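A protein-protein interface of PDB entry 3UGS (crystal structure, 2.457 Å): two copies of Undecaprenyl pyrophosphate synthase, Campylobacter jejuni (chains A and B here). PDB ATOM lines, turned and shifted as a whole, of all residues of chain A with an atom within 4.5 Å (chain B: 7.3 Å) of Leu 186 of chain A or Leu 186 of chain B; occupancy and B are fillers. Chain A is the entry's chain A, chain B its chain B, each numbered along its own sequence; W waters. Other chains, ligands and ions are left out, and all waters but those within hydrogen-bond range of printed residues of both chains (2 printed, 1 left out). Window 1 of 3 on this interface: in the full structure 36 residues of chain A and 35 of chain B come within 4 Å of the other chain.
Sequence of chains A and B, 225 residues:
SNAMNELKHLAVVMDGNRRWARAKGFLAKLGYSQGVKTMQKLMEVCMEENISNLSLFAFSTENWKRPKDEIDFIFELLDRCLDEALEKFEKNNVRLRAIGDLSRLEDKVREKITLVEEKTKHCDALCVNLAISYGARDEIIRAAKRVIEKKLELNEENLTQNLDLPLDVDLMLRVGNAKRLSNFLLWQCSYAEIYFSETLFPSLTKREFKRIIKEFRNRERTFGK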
ATOM      1  N   ALA A 136     -10.584 -28.791 -11.452  1.00  0.00           N
ATOM      2  CA  ALA A 136     -11.904 -28.662 -12.145  1.00  0.00           C
ATOM      3  C   ALA A 136     -12.187 -27.212 -12.451  1.00  0.00           C
ATOM      4  O   ALA A 136     -12.756 -26.874 -13.483  1.00  0.00           O
ATOM      5  CB  ALA A 136     -13.024 -29.242 -11.321  1.00  0.00           C
ATOM      6  N   LEU A 181     -14.599 -33.630  -2.663  1.00  0.00           N
ATOM      7  CA  LEU A 181     -14.238 -33.806  -4.092  1.00  0.00           C
ATOM      8  C   LEU A 181     -12.827 -33.369  -4.465  1.00  0.00           C
ATOM      9  O   LEU A 181     -12.242 -33.811  -5.456  1.00  0.00           O
ATOM     10  CB  LEU A 181     -15.245 -33.110  -4.992  1.00  0.00           C
ATOM     11  CG  LEU A 181     -16.654 -33.729  -4.918  1.00  0.00           C
ATOM     12  CD1 LEU A 181     -17.540 -33.089  -5.991  1.00  0.00           C
ATOM     13  CD2 LEU A 181     -16.634 -35.242  -5.078  1.00  0.00           C
ATOM     14  N   ASN A 183     -11.657 -30.771  -5.871  1.00  0.00           N
ATOM     15  CA  ASN A 183     -11.474 -30.109  -7.163  1.00  0.00           C
ATOM     16  C   ASN A 183     -11.366 -31.086  -8.348  1.00  0.00           C
ATOM     17  O   ASN A 183     -10.734 -30.833  -9.341  1.00  0.00           O
ATOM     18  CB  ASN A 183     -10.226 -29.211  -7.100  1.00  0.00           C
ATOM     19  CG  ASN A 183     -10.238 -28.080  -8.135  1.00  0.00           C
ATOM     20  OD1 ASN A 183     -11.290 -27.740  -8.685  1.00  0.00           O
ATOM     21  ND2 ASN A 183      -9.052 -27.536  -8.443  1.00  0.00           N
ATOM     22  N   PHE A 184     -12.046 -32.201  -8.217  1.00  0.00           N
ATOM     23  CA  PHE A 184     -12.036 -33.268  -9.256  1.00  0.00           C
ATOM     24  C   PHE A 184     -13.358 -33.370 -10.044  1.00  0.00           C
ATOM     25  O   PHE A 184     -14.410 -33.734  -9.516  1.00  0.00           O
ATOM     26  CB  PHE A 184     -11.750 -34.611  -8.604  1.00  0.00           C
ATOM     27  CG  PHE A 184     -11.414 -35.708  -9.568  1.00  0.00           C
ATOM     28  CD1 PHE A 184     -10.563 -35.483 -10.626  1.00  0.00           C
ATOM     29  CD2 PHE A 184     -11.913 -36.970  -9.383  1.00  0.00           C
ATOM     30  CE1 PHE A 184     -10.236 -36.498 -11.499  1.00  0.00           C
ATOM     31  CE2 PHE A 184     -11.587 -38.014 -10.236  1.00  0.00           C
ATOM     32  CZ  PHE A 184     -10.765 -37.765 -11.311  1.00  0.00           C
ATOM     33  N   LEU A 185     -13.266 -33.038 -11.307  1.00  0.00           N
ATOM     34  CA  LEU A 185     -14.406 -33.184 -12.259  1.00  0.00           C
ATOM     35  C   LEU A 185     -15.751 -32.602 -11.742  1.00  0.00           C
ATOM     36  O   LEU A 185     -16.795 -33.221 -11.808  1.00  0.00           O
ATOM     37  CB  LEU A 185     -14.591 -34.647 -12.650  1.00  0.00           C
ATOM     38  CG  LEU A 185     -13.390 -35.275 -13.401  1.00  0.00           C
ATOM     39  CD1 LEU A 185     -13.571 -36.754 -13.740  1.00  0.00           C
ATOM     40  CD2 LEU A 185     -13.079 -34.528 -14.677  1.00  0.00           C
ATOM     41  N   LEU A 186     -15.687 -31.392 -11.217  1.00  0.00           N
ATOM     42  CA  LEU A 186     -16.840 -30.775 -10.492  1.00  0.00           C
ATOM     43  C   LEU A 186     -18.033 -30.639 -11.432  1.00  0.00           C
ATOM     44  O   LEU A 186     -19.145 -31.022 -11.133  1.00  0.00           O
ATOM     45  CB  LEU A 186     -16.508 -29.387  -9.916  1.00  0.00           C
ATOM     46  CG  LEU A 186     -15.381 -29.261  -8.862  1.00  0.00           C
ATOM     47  CD1 LEU A 186     -15.240 -27.793  -8.369  1.00  0.00           C
ATOM     48  CD2 LEU A 186     -15.572 -30.170  -7.660  1.00  0.00           C
ATOM     49  N   TRP A 187     -17.745 -30.016 -12.559  1.00  0.00           N
ATOM     50  CA  TRP A 187     -18.748 -29.726 -13.575  1.00  0.00           C
ATOM     51  C   TRP A 187     -19.425 -31.015 -14.046  1.00  0.00           C
ATOM     52  O   TRP A 187     -20.661 -31.126 -14.166  1.00  0.00           O
ATOM     53  CB  TRP A 187     -18.093 -29.021 -14.745  1.00  0.00           C
ATOM     54  CG  TRP A 187     -19.066 -28.676 -15.836  1.00  0.00           C
ATOM     55  CD1 TRP A 187     -19.586 -29.527 -16.796  1.00  0.00           C
ATOM     56  CD2 TRP A 187     -19.653 -27.363 -16.111  1.00  0.00           C
ATOM     57  NE1 TRP A 187     -20.449 -28.856 -17.620  1.00  0.00           N
ATOM     58  CE2 TRP A 187     -20.553 -27.553 -17.254  1.00  0.00           C
ATOM     59  CE3 TRP A 187     -19.549 -26.107 -15.534  1.00  0.00           C
ATOM     60  CZ2 TRP A 187     -21.294 -26.502 -17.802  1.00  0.00           C
ATOM     61  CZ3 TRP A 187     -20.321 -25.053 -16.067  1.00  0.00           C
ATOM     62  CH2 TRP A 187     -21.177 -25.248 -17.175  1.00  0.00           C
ATOM     63  N   GLN A 188     -18.584 -31.999 -14.297  1.00  0.00           N
ATOM     64  CA  GLN A 188     -19.017 -33.313 -14.789  1.00  0.00           C
ATOM     65  C   GLN A 188     -19.841 -34.090 -13.729  1.00  0.00           C
ATOM     66  O   GLN A 188     -20.619 -35.013 -14.058  1.00  0.00           O
ATOM     67  CB  GLN A 188     -17.848 -34.156 -15.281  1.00  0.00           C
ATOM     68  CG  GLN A 188     -17.095 -33.561 -16.455  1.00  0.00           C
ATOM     69  CD  GLN A 188     -15.928 -32.647 -16.045  1.00  0.00           C
ATOM     70  OE1 GLN A 188     -15.913 -32.068 -14.950  1.00  0.00           O
ATOM     71  NE2 GLN A 188     -14.924 -32.535 -16.916  1.00  0.00           N
ATOM     72  N   CYS A 189     -19.689 -33.666 -12.478  1.00  0.00           N
ATOM     73  CA  CYS A 189     -20.290 -34.355 -11.325  1.00  0.00           C
ATOM     74  C   CYS A 189     -21.605 -33.816 -10.841  1.00  0.00           C
ATOM     75  O   CYS A 189     -22.096 -34.260  -9.775  1.00  0.00           O
ATOM     76  CB  CYS A 189     -19.329 -34.364 -10.124  1.00  0.00           C
ATOM     77  SG  CYS A 189     -18.110 -35.706 -10.169  1.00  0.00           S
ATOM     78  N   SER A 190     -22.179 -32.853 -11.582  1.00  0.00           N
ATOM     79  CA  SER A 190     -23.337 -32.093 -11.058  1.00  0.00           C
ATOM     80  C   SER A 190     -24.357 -33.102 -10.608  1.00  0.00           C
ATOM     81  O   SER A 190     -24.960 -32.934  -9.560  1.00  0.00           O
ATOM     82  CB  SER A 190     -23.998 -31.079 -12.020  1.00  0.00           C
ATOM     83  OG  SER A 190     -24.512 -31.659 -13.214  1.00  0.00           O
ATOM     84  N   TYR B 134     -32.142 -22.167  -9.281  1.00  0.00           N
ATOM     85  CA  TYR B 134     -30.686 -22.091  -9.248  1.00  0.00           C
ATOM     86  C   TYR B 134     -30.029 -23.374  -9.733  1.00  0.00           C
ATOM     87  O   TYR B 134     -30.421 -24.471  -9.415  1.00  0.00           O
ATOM     88  CB  TYR B 134     -30.175 -21.770  -7.847  1.00  0.00           C
ATOM     89  CG  TYR B 134     -28.718 -22.024  -7.684  1.00  0.00           C
ATOM     90  CD1 TYR B 134     -27.798 -20.979  -7.747  1.00  0.00           C
ATOM     91  CD2 TYR B 134     -28.242 -23.312  -7.522  1.00  0.00           C
ATOM     92  CE1 TYR B 134     -26.435 -21.215  -7.621  1.00  0.00           C
ATOM     93  CE2 TYR B 134     -26.903 -23.555  -7.411  1.00  0.00           C
ATOM     94  CZ  TYR B 134     -25.995 -22.513  -7.455  1.00  0.00           C
ATOM     95  OH  TYR B 134     -24.633 -22.788  -7.334  1.00  0.00           O
ATOM     96  N   GLY B 135     -28.982 -23.202 -10.499  1.00  0.00           N
ATOM     97  CA  GLY B 135     -28.109 -24.307 -10.845  1.00  0.00           C
ATOM     98  C   GLY B 135     -26.672 -23.848 -10.858  1.00  0.00           C
ATOM     99  O   GLY B 135     -26.393 -22.695 -11.220  1.00  0.00           O
ATOM    100  N   ALA B 136     -25.768 -24.752 -10.480  1.00  0.00           N
ATOM    101  CA  ALA B 136     -24.325 -24.403 -10.317  1.00  0.00           C
ATOM    102  C   ALA B 136     -23.724 -24.107 -11.659  1.00  0.00           C
ATOM    103  O   ALA B 136     -22.958 -23.183 -11.834  1.00  0.00           O
ATOM    104  CB  ALA B 136     -23.535 -25.511  -9.631  1.00  0.00           C
ATOM    105  N   ARG B 137     -24.092 -24.933 -12.615  1.00  0.00           N
ATOM    106  CA  ARG B 137     -23.546 -24.799 -13.967  1.00  0.00           C
ATOM    107  C   ARG B 137     -23.956 -23.438 -14.549  1.00  0.00           C
ATOM    108  O   ARG B 137     -23.172 -22.722 -15.127  1.00  0.00           O
ATOM    109  CB  ARG B 137     -23.985 -25.940 -14.887  1.00  0.00           C
ATOM    110  CG  ARG B 137     -23.197 -27.229 -14.702  1.00  0.00           C
ATOM    111  CD  ARG B 137     -23.786 -28.349 -15.553  1.00  0.00           C
ATOM    112  NE  ARG B 137     -23.099 -29.648 -15.391  1.00  0.00           N
ATOM    113  CZ  ARG B 137     -23.182 -30.650 -16.267  1.00  0.00           C
ATOM    114  NH1 ARG B 137     -23.904 -30.504 -17.347  1.00  0.00           N
ATOM    115  NH2 ARG B 137     -22.562 -31.801 -16.054  1.00  0.00           N
ATOM    116  N   GLU B 139     -24.987 -20.833 -12.741  1.00  0.00           N
ATOM    117  CA  GLU B 139     -24.321 -19.778 -11.935  1.00  0.00           C
ATOM    118  C   GLU B 139     -22.920 -19.519 -12.512  1.00  0.00           C
ATOM    119  O   GLU B 139     -22.473 -18.389 -12.765  1.00  0.00           O
ATOM    120  CB  GLU B 139     -24.217 -20.172 -10.482  1.00  0.00           C
ATOM    121  CG  GLU B 139     -23.784 -19.008  -9.571  1.00  0.00           C
ATOM    122  CD  GLU B 139     -23.247 -19.464  -8.199  1.00  0.00           C
ATOM    123  OE1 GLU B 139     -23.024 -20.712  -7.965  1.00  0.00           O
ATOM    124  OE2 GLU B 139     -23.020 -18.554  -7.347  1.00  0.00           O
ATOM    125  N   ILE B 140     -22.243 -20.612 -12.786  1.00  0.00           N
ATOM    126  CA  ILE B 140     -20.870 -20.550 -13.342  1.00  0.00           C
ATOM    127  C   ILE B 140     -20.810 -19.802 -14.690  1.00  0.00           C
ATOM    128  O   ILE B 140     -19.925 -18.980 -14.947  1.00  0.00           O
ATOM    129  CB  ILE B 140     -20.221 -21.928 -13.475  1.00  0.00           C
ATOM    130  CG1 ILE B 140     -19.955 -22.519 -12.075  1.00  0.00           C
ATOM    131  CG2 ILE B 140     -18.916 -21.840 -14.269  1.00  0.00           C
ATOM    132  CD1 ILE B 140     -19.372 -23.917 -12.110  1.00  0.00           C
ATOM    133  N   VAL B 169     -17.838 -23.070   0.272  1.00  0.00           N
ATOM    134  CA  VAL B 169     -18.578 -23.934   1.195  1.00  0.00           C
ATOM    135  C   VAL B 169     -17.547 -24.706   2.007  1.00  0.00           C
ATOM    136  O   VAL B 169     -16.627 -25.312   1.482  1.00  0.00           O
ATOM    137  CB  VAL B 169     -19.512 -24.937   0.471  1.00  0.00           C
ATOM    138  CG1 VAL B 169     -19.999 -26.028   1.435  1.00  0.00           C
ATOM    139  CG2 VAL B 169     -20.657 -24.202  -0.235  1.00  0.00           C
ATOM    140  N   MET B 172     -20.814 -29.144   3.325  1.00  0.00           N
ATOM    141  CA  MET B 172     -21.986 -29.524   2.530  1.00  0.00           C
ATOM    142  C   MET B 172     -22.686 -30.712   3.199  1.00  0.00           C
ATOM    143  O   MET B 172     -22.223 -31.838   3.157  1.00  0.00           O
ATOM    144  CB  MET B 172     -21.614 -29.861   1.087  1.00  0.00           C
ATOM    145  CG  MET B 172     -22.764 -30.355   0.225  1.00  0.00           C
ATOM    146  SD  MET B 172     -24.025 -29.114  -0.098  1.00  0.00           S
ATOM    147  CE  MET B 172     -23.370 -28.140  -1.427  1.00  0.00           C
ATOM    148  N   LEU B 181     -24.726 -34.143  -5.285  1.00  0.00           N
ATOM    149  CA  LEU B 181     -24.792 -32.670  -5.058  1.00  0.00           C
ATOM    150  C   LEU B 181     -25.888 -31.983  -5.824  1.00  0.00           C
ATOM    151  O   LEU B 181     -26.281 -30.879  -5.535  1.00  0.00           O
ATOM    152  CB  LEU B 181     -23.466 -31.974  -5.357  1.00  0.00           C
ATOM    153  CG  LEU B 181     -22.297 -32.406  -4.420  1.00  0.00           C
ATOM    154  CD1 LEU B 181     -21.160 -31.406  -4.549  1.00  0.00           C
ATOM    155  CD2 LEU B 181     -22.722 -32.519  -2.969  1.00  0.00           C
ATOM    156  N   SER B 182     -26.352 -32.689  -6.822  1.00  0.00           N
ATOM    157  CA  SER B 182     -27.437 -32.229  -7.677  1.00  0.00           C
ATOM    158  C   SER B 182     -27.335 -30.758  -8.056  1.00  0.00           C
ATOM    159  O   SER B 182     -28.187 -29.955  -7.726  1.00  0.00           O
ATOM    160  CB  SER B 182     -28.774 -32.497  -7.017  1.00  0.00           C
ATOM    161  OG  SER B 182     -28.983 -33.881  -6.992  1.00  0.00           O
ATOM    162  N   ASN B 183     -26.269 -30.426  -8.758  1.00  0.00           N
ATOM    163  CA  ASN B 183     -26.065 -29.060  -9.334  1.00  0.00           C
ATOM    164  C   ASN B 183     -26.103 -27.941  -8.291  1.00  0.00           C
ATOM    165  O   ASN B 183     -26.505 -26.808  -8.560  1.00  0.00           O
ATOM    166  CB  ASN B 183     -27.101 -28.770 -10.422  1.00  0.00           C
ATOM    167  CG  ASN B 183     -26.574 -27.850 -11.523  1.00  0.00           C
ATOM    168  OD1 ASN B 183     -25.389 -27.543 -11.570  1.00  0.00           O
ATOM    169  ND2 ASN B 183     -27.459 -27.401 -12.405  1.00  0.00           N
ATOM    170  N   PHE B 184     -25.688 -28.314  -7.084  1.00  0.00           N
ATOM    171  CA  PHE B 184     -25.701 -27.401  -5.939  1.00  0.00           C
ATOM    172  C   PHE B 184     -24.311 -26.894  -5.596  1.00  0.00           C
ATOM    173  O   PHE B 184     -23.475 -27.617  -5.056  1.00  0.00           O
ATOM    174  CB  PHE B 184     -26.383 -28.035  -4.708  1.00  0.00           C
ATOM    175  CG  PHE B 184     -26.716 -27.048  -3.610  1.00  0.00           C
ATOM    176  CD1 PHE B 184     -27.269 -25.813  -3.890  1.00  0.00           C
ATOM    177  CD2 PHE B 184     -26.485 -27.374  -2.287  1.00  0.00           C
ATOM    178  CE1 PHE B 184     -27.564 -24.920  -2.869  1.00  0.00           C
ATOM    179  CE2 PHE B 184     -26.766 -26.488  -1.269  1.00  0.00           C
ATOM    180  CZ  PHE B 184     -27.313 -25.259  -1.561  1.00  0.00           C
ATOM    181  N   LEU B 185     -24.082 -25.622  -5.918  1.00  0.00           N
ATOM    182  CA  LEU B 185     -22.830 -24.931  -5.507  1.00  0.00           C
ATOM    183  C   LEU B 185     -21.528 -25.711  -5.821  1.00  0.00           C
ATOM    184  O   LEU B 185     -20.572 -25.813  -5.035  1.00  0.00           O
ATOM    185  CB  LEU B 185     -22.857 -24.696  -4.013  1.00  0.00           C
ATOM    186  CG  LEU B 185     -24.032 -23.845  -3.490  1.00  0.00           C
ATOM    187  CD1 LEU B 185     -24.010 -23.834  -1.964  1.00  0.00           C
ATOM    188  CD2 LEU B 185     -23.999 -22.435  -4.101  1.00  0.00           C
ATOM    189  N   LEU B 186     -21.487 -26.257  -7.008  1.00  0.00           N
ATOM    190  CA  LEU B 186     -20.322 -27.092  -7.412  1.00  0.00           C
ATOM    191  C   LEU B 186     -18.970 -26.368  -7.286  1.00  0.00           C
ATOM    192  O   LEU B 186     -17.967 -26.887  -6.786  1.00  0.00           O
ATOM    193  CB  LEU B 186     -20.523 -27.636  -8.811  1.00  0.00           C
ATOM    194  CG  LEU B 186     -21.744 -28.591  -8.920  1.00  0.00           C
ATOM    195  CD1 LEU B 186     -22.068 -28.954 -10.394  1.00  0.00           C
ATOM    196  CD2 LEU B 186     -21.546 -29.850  -8.069  1.00  0.00           C
ATOM    197  N   TRP B 187     -18.937 -25.163  -7.797  1.00  0.00           N
ATOM    198  CA  TRP B 187     -17.680 -24.393  -7.799  1.00  0.00           C
ATOM    199  C   TRP B 187     -17.171 -24.148  -6.382  1.00  0.00           C
ATOM    200  O   TRP B 187     -16.012 -24.385  -6.022  1.00  0.00           O
ATOM    201  CB  TRP B 187     -17.854 -23.079  -8.531  1.00  0.00           C
ATOM    202  CG  TRP B 187     -16.607 -22.241  -8.596  1.00  0.00           C
ATOM    203  CD1 TRP B 187     -16.060 -21.459  -7.612  1.00  0.00           C
ATOM    204  CD2 TRP B 187     -15.733 -22.079  -9.747  1.00  0.00           C
ATOM    205  NE1 TRP B 187     -14.935 -20.847  -8.073  1.00  0.00           N
ATOM    206  CE2 TRP B 187     -14.711 -21.165  -9.347  1.00  0.00           C
ATOM    207  CE3 TRP B 187     -15.741 -22.565 -11.050  1.00  0.00           C
ATOM    208  CZ2 TRP B 187     -13.735 -20.776 -10.196  1.00  0.00           C
ATOM    209  CZ3 TRP B 187     -14.749 -22.202 -11.886  1.00  0.00           C
ATOM    210  CH2 TRP B 187     -13.760 -21.303 -11.479  1.00  0.00           C
ATOM    211  N   GLN B 188     -18.093 -23.678  -5.578  1.00  0.00           N
ATOM    212  CA  GLN B 188     -17.861 -23.360  -4.157  1.00  0.00           C
ATOM    213  C   GLN B 188     -17.433 -24.597  -3.320  1.00  0.00           C
ATOM    214  O   GLN B 188     -16.717 -24.516  -2.313  1.00  0.00           O
ATOM    215  CB  GLN B 188     -19.078 -22.709  -3.556  1.00  0.00           C
ATOM    216  CG  GLN B 188     -19.444 -21.352  -4.143  1.00  0.00           C
ATOM    217  CD  GLN B 188     -20.456 -21.494  -5.297  1.00  0.00           C
ATOM    218  OE1 GLN B 188     -20.632 -22.587  -5.833  1.00  0.00           O
ATOM    219  NE2 GLN B 188     -21.139 -20.388  -5.659  1.00  0.00           N
ATOM    220  N   CYS B 189     -17.852 -25.748  -3.797  1.00  0.00           N
ATOM    221  CA  CYS B 189     -17.653 -27.005  -3.069  1.00  0.00           C
ATOM    222  C   CYS B 189     -16.371 -27.739  -3.430  1.00  0.00           C
ATOM    223  O   CYS B 189     -16.154 -28.865  -3.014  1.00  0.00           O
ATOM    224  CB  CYS B 189     -18.862 -27.941  -3.275  1.00  0.00           C
ATOM    225  SG  CYS B 189     -20.317 -27.515  -2.231  1.00  0.00           S
ATOM    226  N   SER B 190     -15.518 -27.114  -4.222  1.00  0.00           N
ATOM    227  CA  SER B 190     -14.344 -27.837  -4.760  1.00  0.00           C
ATOM    228  C   SER B 190     -13.616 -28.584  -3.658  1.00  0.00           C
ATOM    229  O   SER B 190     -13.269 -29.768  -3.809  1.00  0.00           O
ATOM    230  CB  SER B 190     -13.356 -26.937  -5.511  1.00  0.00           C
ATOM    231  OG  SER B 190     -12.995 -25.840  -4.743  1.00  0.00           O
ATOM    232  N   TYR B 191     -13.393 -27.843  -2.570  1.00  0.00           N
ATOM    233  CA  TYR B 191     -12.777 -28.367  -1.317  1.00  0.00           C
ATOM    234  C   TYR B 191     -13.694 -28.432  -0.057  1.00  0.00           C
ATOM    235  O   TYR B 191     -13.251 -28.598   1.071  1.00  0.00           O
ATOM    236  CB  TYR B 191     -11.517 -27.584  -0.995  1.00  0.00           C
ATOM    237  CG  TYR B 191     -10.396 -28.018  -1.887  1.00  0.00           C
ATOM    238  CD1 TYR B 191      -9.664 -29.183  -1.608  1.00  0.00           C
ATOM    239  CD2 TYR B 191     -10.095 -27.316  -3.039  1.00  0.00           C
ATOM    240  CE1 TYR B 191      -8.645 -29.618  -2.452  1.00  0.00           C
ATOM    241  CE2 TYR B 191      -9.092 -27.750  -3.895  1.00  0.00           C
ATOM    242  CZ  TYR B 191      -8.375 -28.897  -3.591  1.00  0.00           C
ATOM    243  OH  TYR B 191      -7.370 -29.291  -4.451  1.00  0.00           O
ATOM    244  N   ALA B 192     -14.981 -28.307  -0.287  1.00  0.00           N
ATOM    245  CA  ALA B 192     -15.960 -28.456   0.779  1.00  0.00           C
ATOM    246  C   ALA B 192     -15.968 -29.901   1.358  1.00  0.00           C
ATOM    247  O   ALA B 192     -15.923 -30.911   0.658  1.00  0.00           O
ATOM    248  CB  ALA B 192     -17.344 -28.072   0.310  1.00  0.00           C
HETATM  249  O   HOH W   1     -26.367 -30.251 -14.560  1.00  0.00           O
HETATM  250  O   HOH W   2     -23.917 -34.864  -7.584  1.00  0.00           O
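Water W2 lies within hydrogen-bond range of the backbone NH of Leu 181 of chain B, the backbone carbonyl oxygen of Cys 189 of chain A, the backbone carbonyl oxygen of Ser 190 of chain A and the backbone NH of Ser 182 of chain B.
Water W1 bridges the side-chain hydroxyl (OG) of Ser 190 of chain A (2.7 Å) and the guanidinium group (NE) of Arg 137 of chain B (3.4 Å).
Leu 181 of chain A touches Ser 190 of chain B, and with the chains exchanged Ser 190 of chain A touches Leu 181 of chain B.
Asn 183 of chain A touches Ser 190 of chain B, and with the chains exchanged Ser 190 of chain A touches Asn 183 of chain B.
Leu 186 of chain A touches its own counterpart, Leu 186 of chain B.
Leu 186 of chain A touches Ser 190 of chain B, and with the chains exchanged Ser 190 of chain A touches Leu 186 of chain B.
Of the 12 pairs that touch across the chains among the printed residues, 7 have their exchanged pair printed and touching as well.
The backbone NH (N) of Asn 183 of chain B lies within hydrogen-bond range of the backbone carbonyl oxygen (O) of Ser 190 of chain A, at 2.9 Å.
The backbone carbonyl oxygen (O) of Ser 190 of chain B is in hydrogen-bond range of the backbone NH (N) of Asn 183 of chain A (2.8 Å).
The backbone NH (N) of Ser 182 of chain B sits at hydrogen-bond distance from the backbone carbonyl oxygen (O) of Ser 190 of chain A (3.1 Å).
The guanidinium group (NH2) of Arg 137 of chain B lies within hydrogen-bond range of the backbone carbonyl oxygen (O) of Trp 187 of chain A (2.8 Å).
The side-chain hydroxyl of Ser 190 of chain A is in hydrogen-bond range of the guanidinium group of Arg 137 of chain B (3.3 Å).
Leu 186 of chain A touches just these residues of chain B: Leu 186 (3.3 Å) and Ser 190 (3.5 Å).
Printed residues of chain B within 4 Å of Trp 187 of chain A: Arg 137 and Ile 140.
Gln 188 of chain A touches none of the printed residues of chain B.
Printed residues of chain A within 4 Å of Arg 137 of chain B: Trp 187 (2.8 Å) and Ser 190 (3.3 Å).
Val 169 of chain B touches none of the printed residues of chain A.
Printed residues of chain A within 4 Å of Leu 181 of chain B: Ser 190.
Leu 186 of chain B touches just these residues of chain A: Leu 186 (3.3 Å) and Ser 190 (3.3 Å).
Of the printed residues of chain A, Ser 190 of chain B touches Leu 181 (3.7 Å), Asn 183 (2.8 Å) and Leu 186 (3.5 Å).
Of the printed residues of chain A, Tyr 191 of chain B touches Asn 183.
Of the 10 printed residues of chain A, 5 touch a printed residue of chain B.
Hydrophobic or aromatic side chains of chain A that line the printed part of chain B: Leu 186 and Trp 187.
Of the 20 printed residues of chain B, 8 touch a printed residue of chain A.
Printed residues of chain B that touch a printed residue of chain A: Arg 137, Ile 140, Leu 181, Ser 182, Asn 183, Leu 186, Ser 190 and Tyr 191.
Among the printed residues, 12 pairs touch across the chains.
The backbone carbonyl oxygen (O) of Asn 183 of chain B sits at hydrogen-bond distance from the backbone NH (N) of Ala 136 of chain B, at 2.9 Å.
N of Ala 136 of chain A is in hydrogen-bond range of O of Asn 183 of chain A, 2.9 Å away.
N of Arg 137 of chain B lies within hydrogen-bond range of OD1 of Asn 183 of chain B (3.1 Å).
O of Ser 190 of chain B touches C of Leu 181 of chain A, 3.7 Å away.
CB of Asn 183 of chain A touches CE2 of Tyr 191 of chain B, at 3.7 Å.
CD1 of Leu 186 of chain A touches O of Leu 186 of chain B, 3.3 Å away.
Leu 186 of chain A touches Ser 190 of chain B (CD1 to CB, 3.5 Å).
CZ3 of Trp 187 of chain A touches CG2 of Ile 140 of chain B (3.9 Å).
Ser 190 of chain A touches Leu 181 of chain B.
CD1 of Leu 186 of chain B touches CB of Ser 190 of chain A, at 3.3 Å.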
